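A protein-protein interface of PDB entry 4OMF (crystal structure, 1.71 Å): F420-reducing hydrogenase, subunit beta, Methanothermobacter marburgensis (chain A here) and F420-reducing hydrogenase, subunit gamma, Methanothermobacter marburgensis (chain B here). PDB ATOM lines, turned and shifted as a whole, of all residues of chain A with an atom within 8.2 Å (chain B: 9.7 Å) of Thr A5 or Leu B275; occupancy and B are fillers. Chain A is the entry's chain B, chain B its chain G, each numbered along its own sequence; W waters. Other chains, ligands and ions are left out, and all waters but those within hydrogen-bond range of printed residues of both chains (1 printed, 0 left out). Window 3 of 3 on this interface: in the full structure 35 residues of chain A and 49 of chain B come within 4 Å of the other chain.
The chain-end carboxylate (OXT) of Leu B275 lies within salt-bridge range of the side-chain amino group (NZ) of Lys B270, 3.7 Å away.
The guanidinium group of Arg A222 lies within hydrogen-bond range of the backbone carbonyl oxygen of Thr A5.
The guanidinium group of Arg A110 sits at hydrogen-bond distance from the backbone carbonyl oxygen of Leu A202.
The guanidinium group (NH1) of Arg A110 is in salt-bridge range of the side-chain carboxylate (OD1) of Asp A204 (3.1 Å).
Of the 22 printed residues of chain A, 4 touch a printed residue of chain B.
Printed residues of chain A that touch a printed residue of chain B: Thr A5, Arg A110, Glu A201 and Leu A202.
Hydrophobic or aromatic side chains of chain A within 4 Å of the printed part of chain B: Leu A202.
Of the 10 printed residues of chain B, 4 touch a printed residue of chain A.
Printed residues of chain B that touch a printed residue of chain A: Ile B269, Lys B270, Leu B273 and Leu B275.
Hydrophobic or aromatic side chains of chain B that line the printed part of chain A: Ile B269, Leu B273 and Leu B275.
Along chain B the printed residues that touch a printed residue of chain A span positions 269 to 275.
Water W1 lies within hydrogen-bond range of O of Arg A110 (3.3 Å) and O of Ile B269 (3.5 Å).
Thr A5 touches just one residue of chain B: Leu B275.
Leu B275 touches just these residues of chain A: Thr A5 (2.8 Å) and Glu A201 (3.7 Å).
No residue of chain B comes within 4 Å of Gly A4.
No residue of chain A comes within 4 Å of Gly B274.
Printed residues of chain A within 4 Å of Ile B269: Arg A110 (3.8 Å) and Leu A202 (3.9 Å).
Of the printed residues of chain B, Glu A201 touches Leu B275 (3.7 Å).
Leu A3 touches none of the printed residues of chain B.
Tyr A6 touches none of the printed residues of chain B.
The nearest residue of chain B that does not touch Thr A5 is Gly B274 (4.6 Å).
The nearest printed residue of chain A that does not touch Leu B273 is Thr A223 (4.2 Å).
The side-chain hydroxyl (OG1) of Thr A5 lies within hydrogen-bond range of the chain-end carboxylate (OXT) of Leu B275 (2.8 Å).
Among the printed residues, pairs that only touch across the chains: Arg A110 with Leu B273 (3.5 Å), Glu A201 with Leu B275 (3.7 Å), Arg A110 with Ile B269 (3.8 Å), Leu A202 with Ile B269 (3.9 Å), Leu A202 with Lys B270 (3.9 Å) and Leu A202 with Leu B273 (3.99 Å).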
ATOM      1  N   VAL A   2     -15.444  -5.128  -4.431  1.00  0.00           N
ATOM      2  CA  VAL A   2     -16.305  -5.195  -3.253  1.00  0.00           C
ATOM      3  C   VAL A   2     -17.712  -5.629  -3.623  1.00  0.00           C
ATOM      4  O   VAL A   2     -18.587  -5.652  -2.783  1.00  0.00           O
ATOM      5  CB  VAL A   2     -16.405  -3.828  -2.525  1.00  0.00           C
ATOM      6  CG1 VAL A   2     -15.039  -3.371  -2.039  1.00  0.00           C
ATOM      7  CG2 VAL A   2     -17.040  -2.772  -3.442  1.00  0.00           C
ATOM      8  N   LEU A   3     -17.916  -5.960  -4.892  1.00  0.00           N
ATOM      9  CA  LEU A   3     -19.235  -6.303  -5.395  1.00  0.00           C
ATOM     10  C   LEU A   3     -19.345  -7.783  -5.719  1.00  0.00           C
ATOM     11  O   LEU A   3     -20.367  -8.228  -6.214  1.00  0.00           O
ATOM     12  CB  LEU A   3     -19.576  -5.474  -6.642  1.00  0.00           C
ATOM     13  CG  LEU A   3     -19.901  -3.977  -6.474  1.00  0.00           C
ATOM     14  CD1 LEU A   3     -20.392  -3.381  -7.786  1.00  0.00           C
ATOM     15  CD2 LEU A   3     -20.940  -3.754  -5.371  1.00  0.00           C
ATOM     16  N   GLY A   4     -18.298  -8.547  -5.430  1.00  0.00           N
ATOM     17  CA  GLY A   4     -18.301  -9.955  -5.752  1.00  0.00           C
ATOM     18  C   GLY A   4     -18.075 -10.169  -7.239  1.00  0.00           C
ATOM     19  O   GLY A   4     -17.780  -9.232  -7.979  1.00  0.00           O
ATOM     20  N   THR A   5     -18.208 -11.418  -7.666  1.00  0.00           N
ATOM     21  CA  THR A   5     -17.972 -11.797  -9.044  1.00  0.00           C
ATOM     22  C   THR A   5     -19.249 -11.548  -9.827  1.00  0.00           C
ATOM     23  O   THR A   5     -20.333 -11.937  -9.371  1.00  0.00           O
ATOM     24  CB  THR A   5     -17.551 -13.270  -9.132  1.00  0.00           C
ATOM     25  OG1 THR A   5     -16.358 -13.457  -8.360  1.00  0.00           O
ATOM     26  CG2 THR A   5     -17.305 -13.687 -10.577  1.00  0.00           C
ATOM     27  N   TYR A   6     -19.144 -10.872 -10.974  1.00  0.00           N
ATOM     28  CA  TYR A   6     -20.336 -10.652 -11.803  1.00  0.00           C
ATOM     29  C   TYR A   6     -20.037 -10.606 -13.299  1.00  0.00           C
ATOM     30  O   TYR A   6     -18.892 -10.453 -13.710  1.00  0.00           O
ATOM     31  CB  TYR A   6     -21.052  -9.360 -11.402  1.00  0.00           C
ATOM     32  CG  TYR A   6     -20.208  -8.114 -11.494  1.00  0.00           C
ATOM     33  CD1 TYR A   6     -19.545  -7.614 -10.373  1.00  0.00           C
ATOM     34  CD2 TYR A   6     -20.086  -7.423 -12.687  1.00  0.00           C
ATOM     35  CE1 TYR A   6     -18.773  -6.467 -10.447  1.00  0.00           C
ATOM     36  CE2 TYR A   6     -19.297  -6.275 -12.777  1.00  0.00           C
ATOM     37  CZ  TYR A   6     -18.651  -5.807 -11.650  1.00  0.00           C
ATOM     38  OH  TYR A   6     -17.890  -4.673 -11.721  1.00  0.00           O
ATOM     39  N   LYS A   7     -21.087 -10.712 -14.102  1.00  0.00           N
ATOM     40  CA  LYS A   7     -20.940 -10.701 -15.556  1.00  0.00           C
ATOM     41  C   LYS A   7     -21.323  -9.350 -16.122  1.00  0.00           C
ATOM     42  O   LYS A   7     -20.638  -8.802 -16.990  1.00  0.00           O
ATOM     43  CB  LYS A   7     -21.795 -11.805 -16.187  1.00  0.00           C
ATOM     44  CG  LYS A   7     -21.263 -13.215 -15.942  1.00  0.00           C
ATOM     45  CD  LYS A   7     -22.136 -14.282 -16.592  1.00  0.00           C
ATOM     46  CE  LYS A   7     -21.683 -15.678 -16.187  1.00  0.00           C
ATOM     47  NZ  LYS A   7     -20.344 -16.015 -16.718  1.00  0.00           N
ATOM     48  N   GLU A   8     -22.423  -8.800 -15.623  1.00  0.00           N
ATOM     49  CA  GLU A   8     -22.874  -7.491 -16.084  1.00  0.00           C
ATOM     50  C   GLU A   8     -23.677  -6.780 -15.005  1.00  0.00           C
ATOM     51  O   GLU A   8     -24.331  -7.428 -14.201  1.00  0.00           O
ATOM     52  CB  GLU A   8     -23.713  -7.632 -17.355  1.00  0.00           C
ATOM     53  CG  GLU A   8     -23.980  -6.290 -18.031  1.00  0.00           C
ATOM     54  CD  GLU A   8     -24.520  -6.434 -19.439  1.00  0.00           C
ATOM     55  OE1 GLU A   8     -24.626  -7.580 -19.917  1.00  0.00           O
ATOM     56  OE2 GLU A   8     -24.833  -5.395 -20.066  1.00  0.00           O
ATOM     57  N   ILE A   9     -23.598  -5.449 -14.983  1.00  0.00           N
ATOM     58  CA  ILE A   9     -24.424  -4.626 -14.106  1.00  0.00           C
ATOM     59  C   ILE A   9     -25.195  -3.610 -14.944  1.00  0.00           C
ATOM     60  O   ILE A   9     -24.594  -2.877 -15.737  1.00  0.00           O
ATOM     61  CB  ILE A   9     -23.583  -3.873 -13.056  1.00  0.00           C
ATOM     62  CG1 ILE A   9     -22.763  -4.869 -12.222  1.00  0.00           C
ATOM     63  CG2 ILE A   9     -24.492  -3.018 -12.178  1.00  0.00           C
ATOM     64  CD1 ILE A   9     -21.911  -4.212 -11.144  1.00  0.00           C
ATOM     65  N   THR A 106     -29.057 -16.509   1.221  1.00  0.00           N
ATOM     66  CA  THR A 106     -28.335 -17.048   0.083  1.00  0.00           C
ATOM     67  C   THR A 106     -27.186 -17.935   0.585  1.00  0.00           C
ATOM     68  O   THR A 106     -26.887 -18.959   0.001  1.00  0.00           O
ATOM     69  CB  THR A 106     -27.825 -15.905  -0.818  1.00  0.00           C
ATOM     70  OG1 THR A 106     -28.948 -15.140  -1.278  1.00  0.00           O
ATOM     71  CG2 THR A 106     -27.075 -16.426  -2.020  1.00  0.00           C
ATOM     72  N   ARG A 110     -26.527 -21.859  -0.377  1.00  0.00           N
ATOM     73  CA  ARG A 110     -25.345 -22.277  -1.132  1.00  0.00           C
ATOM     74  C   ARG A 110     -24.547 -23.281  -0.297  1.00  0.00           C
ATOM     75  O   ARG A 110     -23.950 -24.221  -0.836  1.00  0.00           O
ATOM     76  CB  ARG A 110     -24.467 -21.070  -1.516  1.00  0.00           C
ATOM     77  CG  ARG A 110     -25.096 -20.090  -2.509  1.00  0.00           C
ATOM     78  CD  ARG A 110     -25.664 -20.777  -3.741  1.00  0.00           C
ATOM     79  NE  ARG A 110     -25.856 -19.819  -4.830  1.00  0.00           N
ATOM     80  CZ  ARG A 110     -26.535 -20.085  -5.940  1.00  0.00           C
ATOM     81  NH1 ARG A 110     -26.672 -19.155  -6.877  1.00  0.00           N
ATOM     82  NH2 ARG A 110     -27.103 -21.273  -6.104  1.00  0.00           N
ATOM     83  N   VAL A 199     -24.331  -7.021  -1.496  1.00  0.00           N
ATOM     84  CA  VAL A 199     -25.055  -7.159  -2.750  1.00  0.00           C
ATOM     85  C   VAL A 199     -25.374  -8.609  -3.100  1.00  0.00           C
ATOM     86  O   VAL A 199     -25.535  -8.939  -4.278  1.00  0.00           O
ATOM     87  CB  VAL A 199     -24.280  -6.512  -3.924  1.00  0.00           C
ATOM     88  CG1 VAL A 199     -24.348  -4.981  -3.843  1.00  0.00           C
ATOM     89  CG2 VAL A 199     -22.830  -6.981  -3.959  1.00  0.00           C
ATOM     90  N   ALA A 200     -25.509  -9.461  -2.086  1.00  0.00           N
ATOM     91  CA  ALA A 200     -25.866 -10.872  -2.303  1.00  0.00           C
ATOM     92  C   ALA A 200     -24.912 -11.501  -3.323  1.00  0.00           C
ATOM     93  O   ALA A 200     -25.323 -11.889  -4.413  1.00  0.00           O
ATOM     94  CB  ALA A 200     -27.321 -11.010  -2.775  1.00  0.00           C
ATOM     95  N   GLU A 201     -23.640 -11.574  -2.956  1.00  0.00           N
ATOM     96  CA  GLU A 201     -22.578 -11.973  -3.864  1.00  0.00           C
ATOM     97  C   GLU A 201     -22.686 -13.395  -4.397  1.00  0.00           C
ATOM     98  O   GLU A 201     -22.057 -13.709  -5.398  1.00  0.00           O
ATOM     99  CB  GLU A 201     -21.226 -11.801  -3.171  1.00  0.00           C
ATOM    100  CG  GLU A 201     -20.938 -10.342  -2.808  1.00  0.00           C
ATOM    101  CD  GLU A 201     -19.680 -10.159  -1.974  1.00  0.00           C
ATOM    102  OE1 GLU A 201     -18.759 -10.996  -2.098  1.00  0.00           O
ATOM    103  OE2 GLU A 201     -19.618  -9.172  -1.197  1.00  0.00           O
ATOM    104  N   LEU A 202     -23.457 -14.262  -3.737  1.00  0.00           N
ATOM    105  CA  LEU A 202     -23.493 -15.659  -4.158  1.00  0.00           C
ATOM    106  C   LEU A 202     -24.775 -16.019  -4.920  1.00  0.00           C
ATOM    107  O   LEU A 202     -24.992 -17.181  -5.262  1.00  0.00           O
ATOM    108  CB  LEU A 202     -23.321 -16.586  -2.939  1.00  0.00           C
ATOM    109  CG  LEU A 202     -21.976 -16.388  -2.207  1.00  0.00           C
ATOM    110  CD1 LEU A 202     -21.841 -17.259  -0.954  1.00  0.00           C
ATOM    111  CD2 LEU A 202     -20.821 -16.640  -3.146  1.00  0.00           C
ATOM    112  N   ALA A 203     -25.628 -15.028  -5.185  1.00  0.00           N
ATOM    113  CA  ALA A 203     -26.886 -15.290  -5.875  1.00  0.00           C
ATOM    114  C   ALA A 203     -26.651 -15.490  -7.372  1.00  0.00           C
ATOM    115  O   ALA A 203     -25.601 -15.111  -7.892  1.00  0.00           O
ATOM    116  CB  ALA A 203     -27.876 -14.141  -5.652  1.00  0.00           C
ATOM    117  N   ASP A 204     -27.627 -16.054  -8.071  1.00  0.00           N
ATOM    118  CA  ASP A 204     -27.530 -16.129  -9.528  1.00  0.00           C
ATOM    119  C   ASP A 204     -27.576 -14.739 -10.175  1.00  0.00           C
ATOM    120  O   ASP A 204     -26.811 -14.458 -11.100  1.00  0.00           O
ATOM    121  CB  ASP A 204     -28.645 -16.972 -10.102  1.00  0.00           C
ATOM    122  CG  ASP A 204     -28.499 -18.434  -9.757  1.00  0.00           C
ATOM    123  OD1 ASP A 204     -27.364 -18.963  -9.843  1.00  0.00           O
ATOM    124  OD2 ASP A 204     -29.518 -19.052  -9.421  1.00  0.00           O
ATOM    125  N   SER A 206     -28.450 -10.608  -8.660  1.00  0.00           N
ATOM    126  CA  SER A 206     -28.681  -9.835  -7.440  1.00  0.00           C
ATOM    127  C   SER A 206     -29.300  -8.476  -7.778  1.00  0.00           C
ATOM    128  O   SER A 206     -28.936  -7.864  -8.778  1.00  0.00           O
ATOM    129  CB  SER A 206     -27.367  -9.632  -6.674  1.00  0.00           C
ATOM    130  OG  SER A 206     -26.682 -10.856  -6.442  1.00  0.00           O
ATOM    131  N   ILE A 220     -27.336  -7.075 -10.975  1.00  0.00           N
ATOM    132  CA  ILE A 220     -26.018  -7.676 -11.148  1.00  0.00           C
ATOM    133  C   ILE A 220     -26.196  -9.140 -11.535  1.00  0.00           C
ATOM    134  O   ILE A 220     -26.682  -9.923 -10.720  1.00  0.00           O
ATOM    135  CB  ILE A 220     -25.214  -7.590  -9.840  1.00  0.00           C
ATOM    136  CG1 ILE A 220     -24.980  -6.131  -9.435  1.00  0.00           C
ATOM    137  CG2 ILE A 220     -23.886  -8.318  -9.990  1.00  0.00           C
ATOM    138  CD1 ILE A 220     -24.471  -5.988  -8.005  1.00  0.00           C
ATOM    139  N   THR A 221     -25.846  -9.517 -12.768  1.00  0.00           N
ATOM    140  CA  THR A 221     -25.918 -10.934 -13.136  1.00  0.00           C
ATOM    141  C   THR A 221     -24.585 -11.588 -12.795  1.00  0.00           C
ATOM    142  O   THR A 221     -23.537 -10.970 -12.945  1.00  0.00           O
ATOM    143  CB  THR A 221     -26.257 -11.160 -14.636  1.00  0.00           C
ATOM    144  OG1 THR A 221     -25.347 -10.432 -15.450  1.00  0.00           O
ATOM    145  CG2 THR A 221     -27.671 -10.684 -14.944  1.00  0.00           C
ATOM    146  N   ARG A 222     -24.621 -12.831 -12.319  1.00  0.00           N
ATOM    147  CA  ARG A 222     -23.419 -13.464 -11.799  1.00  0.00           C
ATOM    148  C   ARG A 222     -23.134 -14.846 -12.398  1.00  0.00           C
ATOM    149  O   ARG A 222     -22.058 -15.071 -12.962  1.00  0.00           O
ATOM    150  CB  ARG A 222     -23.502 -13.581 -10.262  1.00  0.00           C
ATOM    151  CG  ARG A 222     -23.782 -12.268  -9.524  1.00  0.00           C
ATOM    152  CD  ARG A 222     -23.662 -12.433  -7.994  1.00  0.00           C
ATOM    153  NE  ARG A 222     -23.926 -11.174  -7.282  1.00  0.00           N
ATOM    154  CZ  ARG A 222     -23.007 -10.244  -7.038  1.00  0.00           C
ATOM    155  NH1 ARG A 222     -21.741 -10.407  -7.443  1.00  0.00           N
ATOM    156  NH2 ARG A 222     -23.350  -9.138  -6.383  1.00  0.00           N
ATOM    157  N   THR A 223     -24.061 -15.783 -12.265  1.00  0.00           N
ATOM    158  CA  THR A 223     -23.820 -17.146 -12.739  1.00  0.00           C
ATOM    159  C   THR A 223     -24.335 -17.300 -14.168  1.00  0.00           C
ATOM    160  O   THR A 223     -25.060 -16.435 -14.655  1.00  0.00           O
ATOM    161  CB  THR A 223     -24.513 -18.168 -11.863  1.00  0.00           C
ATOM    162  OG1 THR A 223     -25.921 -17.911 -11.915  1.00  0.00           O
ATOM    163  CG2 THR A 223     -24.034 -18.081 -10.413  1.00  0.00           C
ATOM    164  N   ASP A 224     -23.973 -18.395 -14.841  1.00  0.00           N
ATOM    165  CA  ASP A 224     -24.502 -18.655 -16.182  1.00  0.00           C
ATOM    166  C   ASP A 224     -26.040 -18.636 -16.182  1.00  0.00           C
ATOM    167  O   ASP A 224     -26.659 -18.051 -17.073  1.00  0.00           O
ATOM    168  CB  ASP A 224     -23.996 -20.000 -16.733  1.00  0.00           C
ATOM    169  CG  ASP A 224     -22.492 -20.004 -17.010  1.00  0.00           C
ATOM    170  OD1 ASP A 224     -21.866 -18.920 -16.987  1.00  0.00           O
ATOM    171  OD2 ASP A 224     -21.935 -21.099 -17.263  1.00  0.00           O
ATOM    172  N   GLU B 266     -16.405 -20.820   2.532  1.00  0.00           N
ATOM    173  CA  GLU B 266     -16.604 -19.877   1.445  1.00  0.00           C
ATOM    174  C   GLU B 266     -15.891 -20.292   0.148  1.00  0.00           C
ATOM    175  O   GLU B 266     -16.469 -20.204  -0.929  1.00  0.00           O
ATOM    176  CB  GLU B 266     -16.147 -18.487   1.862  1.00  0.00           C
ATOM    177  CG  GLU B 266     -16.500 -17.415   0.857  1.00  0.00           C
ATOM    178  CD  GLU B 266     -16.347 -16.026   1.441  1.00  0.00           C
ATOM    179  OE1 GLU B 266     -15.233 -15.473   1.354  1.00  0.00           O
ATOM    180  OE2 GLU B 266     -17.330 -15.512   2.016  1.00  0.00           O
ATOM    181  N   GLU B 267     -14.649 -20.744   0.247  1.00  0.00           N
ATOM    182  CA  GLU B 267     -13.880 -21.015  -0.960  1.00  0.00           C
ATOM    183  C   GLU B 267     -14.468 -22.175  -1.759  1.00  0.00           C
ATOM    184  O   GLU B 267     -14.580 -22.117  -2.995  1.00  0.00           O
ATOM    185  CB  GLU B 267     -12.416 -21.296  -0.607  1.00  0.00           C
ATOM    186  CG  GLU B 267     -11.618 -20.030  -0.336  1.00  0.00           C
ATOM    187  CD  GLU B 267     -11.713 -19.013  -1.479  1.00  0.00           C
ATOM    188  OE1 GLU B 267     -11.182 -19.289  -2.576  1.00  0.00           O
ATOM    189  OE2 GLU B 267     -12.326 -17.941  -1.281  1.00  0.00           O
ATOM    190  N   GLN B 268     -14.883 -23.213  -1.054  1.00  0.00           N
ATOM    191  CA  GLN B 268     -15.495 -24.348  -1.728  1.00  0.00           C
ATOM    192  C   GLN B 268     -16.855 -23.967  -2.329  1.00  0.00           C
ATOM    193  O   GLN B 268     -17.197 -24.411  -3.428  1.00  0.00           O
ATOM    194  CB  GLN B 268     -15.634 -25.529  -0.775  1.00  0.00           C
ATOM    195  CG  GLN B 268     -16.123 -26.776  -1.456  1.00  0.00           C
ATOM    196  CD  GLN B 268     -15.081 -27.368  -2.398  1.00  0.00           C
ATOM    197  OE1 GLN B 268     -13.887 -27.296  -2.135  1.00  0.00           O
ATOM    198  NE2 GLN B 268     -15.539 -27.934  -3.509  1.00  0.00           N
ATOM    199  N   ILE B 269     -17.625 -23.137  -1.629  1.00  0.00           N
ATOM    200  CA  ILE B 269     -18.906 -22.698  -2.168  1.00  0.00           C
ATOM    201  C   ILE B 269     -18.709 -21.913  -3.471  1.00  0.00           C
ATOM    202  O   ILE B 269     -19.372 -22.186  -4.468  1.00  0.00           O
ATOM    203  CB  ILE B 269     -19.678 -21.860  -1.133  1.00  0.00           C
ATOM    204  CG1 ILE B 269     -20.311 -22.793  -0.088  1.00  0.00           C
ATOM    205  CG2 ILE B 269     -20.689 -20.922  -1.822  1.00  0.00           C
ATOM    206  CD1 ILE B 269     -20.958 -22.059   1.077  1.00  0.00           C
ATOM    207  N   LYS B 270     -17.769 -20.969  -3.472  1.00  0.00           N
ATOM    208  CA  LYS B 270     -17.528 -20.136  -4.638  1.00  0.00           C
ATOM    209  C   LYS B 270     -16.949 -20.979  -5.776  1.00  0.00           C
ATOM    210  O   LYS B 270     -17.275 -20.766  -6.943  1.00  0.00           O
ATOM    211  CB  LYS B 270     -16.570 -18.985  -4.313  1.00  0.00           C
ATOM    212  CG  LYS B 270     -17.109 -17.974  -3.299  1.00  0.00           C
ATOM    213  CD  LYS B 270     -16.116 -16.849  -3.043  1.00  0.00           C
ATOM    214  CE  LYS B 270     -16.039 -15.896  -4.241  1.00  0.00           C
ATOM    215  NZ  LYS B 270     -15.043 -14.814  -4.052  1.00  0.00           N
ATOM    216  N   LYS B 271     -16.104 -21.940  -5.428  1.00  0.00           N
ATOM    217  CA  LYS B 271     -15.502 -22.798  -6.450  1.00  0.00           C
ATOM    218  C   LYS B 271     -16.587 -23.485  -7.269  1.00  0.00           C
ATOM    219  O   LYS B 271     -16.530 -23.500  -8.511  1.00  0.00           O
ATOM    220  CB  LYS B 271     -14.576 -23.842  -5.820  1.00  0.00           C
ATOM    221  CG  LYS B 271     -14.064 -24.889  -6.804  1.00  0.00           C
ATOM    222  CD  LYS B 271     -13.135 -25.884  -6.123  1.00  0.00           C
ATOM    223  CE  LYS B 271     -12.897 -27.102  -7.015  1.00  0.00           C
ATOM    224  NZ  LYS B 271     -11.763 -27.943  -6.528  1.00  0.00           N
ATOM    225  N   GLU B 272     -17.581 -24.023  -6.577  1.00  0.00           N
ATOM    226  CA  GLU B 272     -18.640 -24.785  -7.227  1.00  0.00           C
ATOM    227  C   GLU B 272     -19.604 -23.895  -8.004  1.00  0.00           C
ATOM    228  O   GLU B 272     -20.243 -24.352  -8.940  1.00  0.00           O
ATOM    229  CB  GLU B 272     -19.408 -25.612  -6.199  1.00  0.00           C
ATOM    230  CG  GLU B 272     -18.541 -26.656  -5.498  1.00  0.00           C
ATOM    231  CD  GLU B 272     -19.356 -27.732  -4.784  1.00  0.00           C
ATOM    232  OE1 GLU B 272     -20.594 -27.565  -4.639  1.00  0.00           O
ATOM    233  OE2 GLU B 272     -18.750 -28.753  -4.372  1.00  0.00           O
ATOM    234  N   LEU B 273     -19.693 -22.624  -7.624  1.00  0.00           N
ATOM    235  CA  LEU B 273     -20.565 -21.666  -8.321  1.00  0.00           C
ATOM    236  C   LEU B 273     -19.857 -21.007  -9.488  1.00  0.00           C
ATOM    237  O   LEU B 273     -20.496 -20.384 -10.335  1.00  0.00           O
ATOM    238  CB  LEU B 273     -21.055 -20.590  -7.351  1.00  0.00           C
ATOM    239  CG  LEU B 273     -22.116 -21.070  -6.359  1.00  0.00           C
ATOM    240  CD1 LEU B 273     -22.273 -20.098  -5.210  1.00  0.00           C
ATOM    241  CD2 LEU B 273     -23.445 -21.274  -7.110  1.00  0.00           C
ATOM    242  N   GLY B 274     -18.533 -21.130  -9.513  1.00  0.00           N
ATOM    243  CA  GLY B 274     -17.719 -20.509 -10.541  1.00  0.00           C
ATOM    244  C   GLY B 274     -17.554 -19.035 -10.255  1.00  0.00           C
ATOM    245  O   GLY B 274     -17.352 -18.239 -11.163  1.00  0.00           O
ATOM    246  N   LEU B 275     -17.652 -18.670  -8.981  1.00  0.00           N
ATOM    247  CA  LEU B 275     -17.462 -17.281  -8.553  1.00  0.00           C
ATOM    248  C   LEU B 275     -16.114 -17.133  -7.829  1.00  0.00           C
ATOM    249  O   LEU B 275     -15.432 -18.133  -7.574  1.00  0.00           O
ATOM    250  CB  LEU B 275     -18.626 -16.831  -7.654  1.00  0.00           C
ATOM    251  CG  LEU B 275     -20.016 -16.998  -8.294  1.00  0.00           C
ATOM    252  CD1 LEU B 275     -21.162 -16.758  -7.313  1.00  0.00           C
ATOM    253  CD2 LEU B 275     -20.169 -16.108  -9.534  1.00  0.00           C
ATOM    254  OXT LEU B 275     -15.652 -16.032  -7.502  1.00  0.00           O
HETATM  255  O   HOH W   1     -22.498 -23.532  -3.723  1.00  0.00           O
